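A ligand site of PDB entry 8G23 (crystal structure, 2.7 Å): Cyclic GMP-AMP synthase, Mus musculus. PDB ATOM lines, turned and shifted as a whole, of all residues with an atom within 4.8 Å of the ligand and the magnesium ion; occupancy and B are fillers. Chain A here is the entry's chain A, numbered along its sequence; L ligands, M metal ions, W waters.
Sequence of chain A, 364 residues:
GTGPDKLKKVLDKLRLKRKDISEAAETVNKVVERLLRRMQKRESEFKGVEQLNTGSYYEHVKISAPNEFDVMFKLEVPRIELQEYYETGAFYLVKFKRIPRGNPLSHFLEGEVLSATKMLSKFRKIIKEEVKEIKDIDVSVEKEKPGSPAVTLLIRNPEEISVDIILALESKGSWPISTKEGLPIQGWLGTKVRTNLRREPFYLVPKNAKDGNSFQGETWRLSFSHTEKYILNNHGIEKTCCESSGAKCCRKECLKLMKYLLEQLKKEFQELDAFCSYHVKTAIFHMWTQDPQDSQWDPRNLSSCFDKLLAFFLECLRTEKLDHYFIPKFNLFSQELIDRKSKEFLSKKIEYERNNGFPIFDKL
OE1 of Glu 228 is in hydrogen-bond range of O13 of the ligand (2.6 Å). The backbone NH of Ser 56 lies close to an oxygen (O5) of the ligand, at 2.9 Å. The side-chain hydroxyl (OG) of Ser 56 lies within hydrogen-bond range of an oxygen (O2) of the ligand (2.6 Å). The side-chain hydroxyl (OG) of Ser 225 sits at hydrogen-bond distance from an oxygen (O13) of the ligand. NZ of Lys 259 is in salt-bridge range of O2 of the ligand, 2.8 Å away. An oxygen (O1) of the ligand sits at hydrogen-bond distance from the side-chain hydroxyl (OG) of Ser 277, at 2.9 Å. A nitrogen (N5) of the ligand sits close to the guanidinium group (NH1) of Arg 221 (3.3 Å). O12 of the ligand sits at hydrogen-bond distance from NZ of Lys 281 (3.2 Å).
The side-chain carboxylate of Glu 228 is in salt-bridge range of the side-chain amino group of Lys 281 (2.7 Å). The side-chain carboxylate of Glu 228 is in hydrogen-bond range of the side-chain hydroxyl of Tyr 278 (2.6 Å). O of Ser 56 is in hydrogen-bond range of N of Lys 62. The side-chain amino group (NZ) of Lys 281 is in salt-bridge range of the side-chain carboxylate (OE2) of Glu 59 (2.6 Å). SG of Cys 276 sits close to N of Tyr 278, 3.6 Å away.
Gly 55 touches the ligand. CD of Lys 62 touches O2 of the ligand, at 3.9 Å. Tyr 278 touches the ligand. Hydrophobic or aromatic side chains that line the ligand: Tyr 278. 12 residues have an atom within 4 Å of the ligand: Gly 55, Ser 56, Lys 62, Glu 68, Asp 70, Arg 221, Ser 225, Glu 228, Lys 259, Ser 277, Tyr 278 and Lys 281. Along chain A the residues within 4 Å of the ligand span positions 55 to 281.
Ser 56 touches the magnesium ion (OG to MG, 3.9 Å). Within 4 Å of the magnesium ion: Ser 56, Glu 68 and Asp 70. Along chain A the residues within 4 Å of the magnesium ion span positions 56 to 70. The nearest printed residue that does not touch the magnesium ion is Gly 55 (4.8 Å).
The magnesium ion is bound by O3 of the ligand (1.9 Å), OE1 of Glu 68 (2.2 Å), water W2 (2.2 Å), O5 of the ligand (2.3 Å), OD2 of Asp 70 (2.4 Å) and O8 of the ligand (2.4 Å).
Water W2 lies within hydrogen-bond range of the side-chain hydroxyl (OG) of Ser 56 (2.7 Å) and the backbone carbonyl oxygen (O) of Glu 68 (2.8 Å). Water W1 lies within hydrogen-bond range of an oxygen (O2) of the ligand (2.6 Å), the side-chain amino group (NZ) of Lys 62 (3.1 Å) and the side-chain carboxylate (OE2) of Glu 263 (3.2 Å).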
ATOM      1  N   GLY A  55      16.557   6.386   0.055  1.00  0.00           N
ATOM      2  CA  GLY A  55      16.412   5.194  -0.748  1.00  0.00           C
ATOM      3  C   GLY A  55      17.148   5.278  -2.063  1.00  0.00           C
ATOM      4  O   GLY A  55      17.823   6.249  -2.380  1.00  0.00           O
ATOM      5  N   SER A  56      17.006   4.214  -2.857  1.00  0.00           N
ATOM      6  CA  SER A  56      17.949   4.060  -3.954  1.00  0.00           C
ATOM      7  C   SER A  56      17.759   5.113  -5.029  1.00  0.00           C
ATOM      8  O   SER A  56      18.743   5.485  -5.690  1.00  0.00           O
ATOM      9  CB  SER A  56      17.867   2.628  -4.550  1.00  0.00           C
ATOM     10  OG  SER A  56      16.573   2.295  -5.055  1.00  0.00           O
ATOM     11  N   GLU A  59      19.703   8.074  -4.122  1.00  0.00           N
ATOM     12  CA  GLU A  59      21.114   7.687  -4.125  1.00  0.00           C
ATOM     13  C   GLU A  59      21.656   7.450  -5.542  1.00  0.00           C
ATOM     14  O   GLU A  59      22.876   7.272  -5.698  1.00  0.00           O
ATOM     15  CB  GLU A  59      21.303   6.426  -3.292  1.00  0.00           C
ATOM     16  CG  GLU A  59      21.024   6.603  -1.809  1.00  0.00           C
ATOM     17  CD  GLU A  59      20.796   5.261  -1.109  1.00  0.00           C
ATOM     18  OE1 GLU A  59      20.695   4.255  -1.856  1.00  0.00           O
ATOM     19  OE2 GLU A  59      20.742   5.206   0.152  1.00  0.00           O
ATOM     20  N   LYS A  62      18.901   3.277  -8.009  1.00  0.00           N
ATOM     21  CA  LYS A  62      17.682   2.618  -8.466  1.00  0.00           C
ATOM     22  C   LYS A  62      17.870   2.043  -9.860  1.00  0.00           C
ATOM     23  O   LYS A  62      18.376   2.721 -10.754  1.00  0.00           O
ATOM     24  CB  LYS A  62      16.536   3.617  -8.488  1.00  0.00           C
ATOM     25  CG  LYS A  62      15.228   3.023  -8.972  1.00  0.00           C
ATOM     26  CD  LYS A  62      14.634   2.181  -7.874  1.00  0.00           C
ATOM     27  CE  LYS A  62      13.305   1.602  -8.269  1.00  0.00           C
ATOM     28  NZ  LYS A  62      13.399   0.366  -9.070  1.00  0.00           N
ATOM     29  N   GLU A  68       9.852   2.954  -7.739  1.00  0.00           N
ATOM     30  CA  GLU A  68       9.755   2.789  -6.290  1.00  0.00           C
ATOM     31  C   GLU A  68      10.531   3.891  -5.599  1.00  0.00           C
ATOM     32  O   GLU A  68      11.769   3.927  -5.659  1.00  0.00           O
ATOM     33  CB  GLU A  68      10.263   1.413  -5.875  1.00  0.00           C
ATOM     34  CG  GLU A  68       9.671   0.926  -4.581  1.00  0.00           C
ATOM     35  CD  GLU A  68      10.460   1.395  -3.360  1.00  0.00           C
ATOM     36  OE1 GLU A  68      11.514   2.055  -3.541  1.00  0.00           O
ATOM     37  OE2 GLU A  68      10.054   1.072  -2.213  1.00  0.00           O
ATOM     38  N   ASP A  70      11.099   6.290  -1.886  1.00  0.00           N
ATOM     39  CA  ASP A  70      10.988   6.213  -0.431  1.00  0.00           C
ATOM     40  C   ASP A  70      11.173   7.588   0.206  1.00  0.00           C
ATOM     41  O   ASP A  70      12.205   8.238  -0.025  1.00  0.00           O
ATOM     42  CB  ASP A  70      12.009   5.250   0.173  1.00  0.00           C
ATOM     43  CG  ASP A  70      12.076   3.937  -0.554  1.00  0.00           C
ATOM     44  OD1 ASP A  70      11.122   3.144  -0.483  1.00  0.00           O
ATOM     45  OD2 ASP A  70      13.121   3.671  -1.175  1.00  0.00           O
ATOM     46  N   ASP A 164       6.858   4.583  -0.645  1.00  0.00           N
ATOM     47  CA  ASP A 164       6.844   4.253   0.777  1.00  0.00           C
ATOM     48  C   ASP A 164       6.904   5.569   1.559  1.00  0.00           C
ATOM     49  O   ASP A 164       7.948   6.235   1.570  1.00  0.00           O
ATOM     50  CB  ASP A 164       8.035   3.368   1.147  1.00  0.00           C
ATOM     51  CG  ASP A 164       7.899   1.941   0.618  1.00  0.00           C
ATOM     52  OD1 ASP A 164       6.765   1.463   0.443  1.00  0.00           O
ATOM     53  OD2 ASP A 164       8.958   1.303   0.381  1.00  0.00           O
ATOM     54  N   ARG A 221      12.360   1.044  15.642  1.00  0.00           N
ATOM     55  CA  ARG A 221      13.648   0.636  15.080  1.00  0.00           C
ATOM     56  C   ARG A 221      14.471   1.850  14.666  1.00  0.00           C
ATOM     57  O   ARG A 221      13.939   2.825  14.121  1.00  0.00           O
ATOM     58  CB  ARG A 221      13.479  -0.292  13.844  1.00  0.00           C
ATOM     59  CG  ARG A 221      14.830  -0.904  13.392  1.00  0.00           C
ATOM     60  CD  ARG A 221      14.848  -1.775  12.103  1.00  0.00           C
ATOM     61  NE  ARG A 221      13.771  -1.582  11.134  1.00  0.00           N
ATOM     62  CZ  ARG A 221      13.870  -0.782  10.079  1.00  0.00           C
ATOM     63  NH1 ARG A 221      14.884   0.055   9.937  1.00  0.00           N
ATOM     64  NH2 ARG A 221      12.933  -0.847   9.114  1.00  0.00           N
ATOM     65  N   SER A 225      18.756   6.015   7.204  1.00  0.00           N
ATOM     66  CA  SER A 225      18.613   6.250   5.767  1.00  0.00           C
ATOM     67  C   SER A 225      19.294   7.523   5.335  1.00  0.00           C
ATOM     68  O   SER A 225      19.849   7.589   4.229  1.00  0.00           O
ATOM     69  CB  SER A 225      17.140   6.300   5.392  1.00  0.00           C
ATOM     70  OG  SER A 225      16.530   5.063   5.637  1.00  0.00           O
ATOM     71  N   GLU A 228      23.083   6.841   5.244  1.00  0.00           N
ATOM     72  CA  GLU A 228      23.401   6.040   4.060  1.00  0.00           C
ATOM     73  C   GLU A 228      23.295   6.859   2.782  1.00  0.00           C
ATOM     74  O   GLU A 228      24.086   6.674   1.841  1.00  0.00           O
ATOM     75  CB  GLU A 228      22.491   4.822   4.008  1.00  0.00           C
ATOM     76  CG  GLU A 228      22.478   4.082   5.311  1.00  0.00           C
ATOM     77  CD  GLU A 228      21.335   3.111   5.418  1.00  0.00           C
ATOM     78  OE1 GLU A 228      20.620   2.885   4.405  1.00  0.00           O
ATOM     79  OE2 GLU A 228      21.157   2.570   6.531  1.00  0.00           O
ATOM     80  N   LYS A 259      22.223  -5.561  -6.564  1.00  0.00           N
ATOM     81  CA  LYS A 259      20.785  -5.374  -6.396  1.00  0.00           C
ATOM     82  C   LYS A 259      20.027  -6.180  -7.440  1.00  0.00           C
ATOM     83  O   LYS A 259      18.999  -6.790  -7.131  1.00  0.00           O
ATOM     84  CB  LYS A 259      20.433  -3.893  -6.522  1.00  0.00           C
ATOM     85  CG  LYS A 259      20.839  -3.050  -5.333  1.00  0.00           C
ATOM     86  CD  LYS A 259      20.838  -1.579  -5.712  1.00  0.00           C
ATOM     87  CE  LYS A 259      19.415  -1.034  -5.887  1.00  0.00           C
ATOM     88  NZ  LYS A 259      18.695  -0.902  -4.582  1.00  0.00           N
ATOM     89  N   GLU A 263      17.273  -9.024  -7.207  1.00  0.00           N
ATOM     90  CA  GLU A 263      15.924  -8.766  -7.727  1.00  0.00           C
ATOM     91  C   GLU A 263      15.477  -9.860  -8.689  1.00  0.00           C
ATOM     92  O   GLU A 263      14.402 -10.452  -8.513  1.00  0.00           O
ATOM     93  CB  GLU A 263      15.873  -7.404  -8.420  1.00  0.00           C
ATOM     94  CG  GLU A 263      15.591  -6.234  -7.529  1.00  0.00           C
ATOM     95  CD  GLU A 263      15.391  -4.983  -8.346  1.00  0.00           C
ATOM     96  OE1 GLU A 263      15.091  -5.126  -9.548  1.00  0.00           O
ATOM     97  OE2 GLU A 263      15.561  -3.851  -7.808  1.00  0.00           O
ATOM     98  N   CYS A 276      16.389  -9.092   1.258  1.00  0.00           N
ATOM     99  CA  CYS A 276      15.979  -7.804   0.721  1.00  0.00           C
ATOM    100  C   CYS A 276      17.208  -7.034   0.250  1.00  0.00           C
ATOM    101  O   CYS A 276      18.354  -7.440   0.524  1.00  0.00           O
ATOM    102  CB  CYS A 276      15.206  -6.977   1.759  1.00  0.00           C
ATOM    103  SG  CYS A 276      16.199  -6.474   3.156  1.00  0.00           S
ATOM    104  N   SER A 277      16.989  -5.918  -0.449  1.00  0.00           N
ATOM    105  CA  SER A 277      18.130  -5.215  -0.992  1.00  0.00           C
ATOM    106  C   SER A 277      18.961  -4.539   0.107  1.00  0.00           C
ATOM    107  O   SER A 277      20.145  -4.271  -0.134  1.00  0.00           O
ATOM    108  CB  SER A 277      17.701  -4.198  -2.036  1.00  0.00           C
ATOM    109  OG  SER A 277      16.797  -3.273  -1.483  1.00  0.00           O
ATOM    110  N   TYR A 278      18.387  -4.295   1.289  1.00  0.00           N
ATOM    111  CA  TYR A 278      19.191  -3.749   2.386  1.00  0.00           C
ATOM    112  C   TYR A 278      20.339  -4.673   2.729  1.00  0.00           C
ATOM    113  O   TYR A 278      21.410  -4.212   3.179  1.00  0.00           O
ATOM    114  CB  TYR A 278      18.347  -3.501   3.635  1.00  0.00           C
ATOM    115  CG  TYR A 278      19.071  -2.590   4.603  1.00  0.00           C
ATOM    116  CD1 TYR A 278      19.344  -1.275   4.261  1.00  0.00           C
ATOM    117  CD2 TYR A 278      19.528  -3.061   5.839  1.00  0.00           C
ATOM    118  CE1 TYR A 278      20.019  -0.415   5.108  1.00  0.00           C
ATOM    119  CE2 TYR A 278      20.211  -2.198   6.723  1.00  0.00           C
ATOM    120  CZ  TYR A 278      20.450  -0.875   6.333  1.00  0.00           C
ATOM    121  OH  TYR A 278      21.123   0.021   7.130  1.00  0.00           O
ATOM    122  N   LYS A 281      22.996  -3.880   0.272  1.00  0.00           N
ATOM    123  CA  LYS A 281      23.506  -2.548   0.624  1.00  0.00           C
ATOM    124  C   LYS A 281      24.457  -2.634   1.808  1.00  0.00           C
ATOM    125  O   LYS A 281      25.462  -1.905   1.865  1.00  0.00           O
ATOM    126  CB  LYS A 281      22.364  -1.607   0.973  1.00  0.00           C
ATOM    127  CG  LYS A 281      22.659  -0.124   0.816  1.00  0.00           C
ATOM    128  CD  LYS A 281      21.622   0.722   1.551  1.00  0.00           C
ATOM    129  CE  LYS A 281      21.451   2.073   0.875  1.00  0.00           C
ATOM    130  NZ  LYS A 281      20.872   3.162   1.727  1.00  0.00           N
ATOM    131  N   HIS A 324      24.837  -5.331  11.069  1.00  0.00           N
ATOM    132  CA  HIS A 324      24.335  -4.020  10.704  1.00  0.00           C
ATOM    133  C   HIS A 324      25.518  -3.061  10.657  1.00  0.00           C
ATOM    134  O   HIS A 324      26.367  -3.063  11.552  1.00  0.00           O
ATOM    135  CB  HIS A 324      23.285  -3.560  11.721  1.00  0.00           C
ATOM    136  CG  HIS A 324      22.388  -2.468  11.223  1.00  0.00           C
ATOM    137  ND1 HIS A 324      22.836  -1.193  10.977  1.00  0.00           N
ATOM    138  CD2 HIS A 324      21.070  -2.470  10.924  1.00  0.00           C
ATOM    139  CE1 HIS A 324      21.830  -0.450  10.541  1.00  0.00           C
ATOM    140  NE2 HIS A 324      20.752  -1.205  10.511  1.00  0.00           N
HETATM  141  P1  LIG L   1      15.386  -0.539  -3.773  1.00  0.00           P
HETATM  142  O1  LIG L   1      15.142  -1.972  -3.419  1.00  0.00           O
HETATM  143  O2  LIG L   1      16.009  -0.284  -5.172  1.00  0.00           O
HETATM  144  O3  LIG L   1      14.107   0.311  -3.647  1.00  0.00           O
HETATM  145  P2  LIG L   1      16.371   0.891  -1.333  1.00  0.00           P
HETATM  146  O4  LIG L   1      17.759   1.112  -0.807  1.00  0.00           O
HETATM  147  O5  LIG L   1      15.516   2.160  -1.503  1.00  0.00           O
HETATM  148  O6  LIG L   1      16.402   0.134  -2.750  1.00  0.00           O
HETATM  149  P3  LIG L   1      14.108  -0.148   0.232  1.00  0.00           P
HETATM  150  O7  LIG L   1      13.691  -1.551   0.479  1.00  0.00           O
HETATM  151  O8  LIG L   1      13.197   0.737  -0.634  1.00  0.00           O
HETATM  152  O9  LIG L   1      15.513  -0.134  -0.475  1.00  0.00           O
HETATM  153  O10 LIG L   1      14.406   0.571   1.606  1.00  0.00           O
HETATM  154  C1  LIG L   1      14.495   2.010   1.697  1.00  0.00           C
HETATM  155  C2  LIG L   1      15.518   2.415   2.738  1.00  0.00           C
HETATM  156  O11 LIG L   1      15.054   2.045   4.064  1.00  0.00           O
HETATM  157  C3  LIG L   1      16.905   1.775   2.607  1.00  0.00           C
HETATM  158  O12 LIG L   1      17.753   2.492   1.716  1.00  0.00           O
HETATM  159  C4  LIG L   1      17.417   1.796   4.056  1.00  0.00           C
HETATM  160  O13 LIG L   1      18.009   3.051   4.388  1.00  0.00           O
HETATM  161  C5  LIG L   1      16.127   1.541   4.843  1.00  0.00           C
HETATM  162  N1  LIG L   1      15.860   0.125   5.133  1.00  0.00           N
HETATM  163  C6  LIG L   1      15.185  -0.779   4.343  1.00  0.00           C
HETATM  164  N2  LIG L   1      15.087  -1.987   4.860  1.00  0.00           N
HETATM  165  C7  LIG L   1      15.764  -1.874   6.073  1.00  0.00           C
HETATM  166  C8  LIG L   1      16.039  -2.805   7.096  1.00  0.00           C
HETATM  167  N3  LIG L   1      15.654  -4.090   7.052  1.00  0.00           N
HETATM  168  N4  LIG L   1      16.743  -2.361   8.170  1.00  0.00           N
HETATM  169  C9  LIG L   1      17.150  -1.092   8.201  1.00  0.00           C
HETATM  170  N5  LIG L   1      16.943  -0.124   7.303  1.00  0.00           N
HETATM  171  C10 LIG L   1      16.242  -0.579   6.248  1.00  0.00           C
HETATM  172 MG    MG M   1      13.535   1.919  -2.704  1.00  0.00          MG
HETATM  173  O   HOH W   1      16.042  -0.696  -7.762  1.00  0.00           O
HETATM  174  O   HOH W   2      14.145   3.268  -4.331  1.00  0.00           O
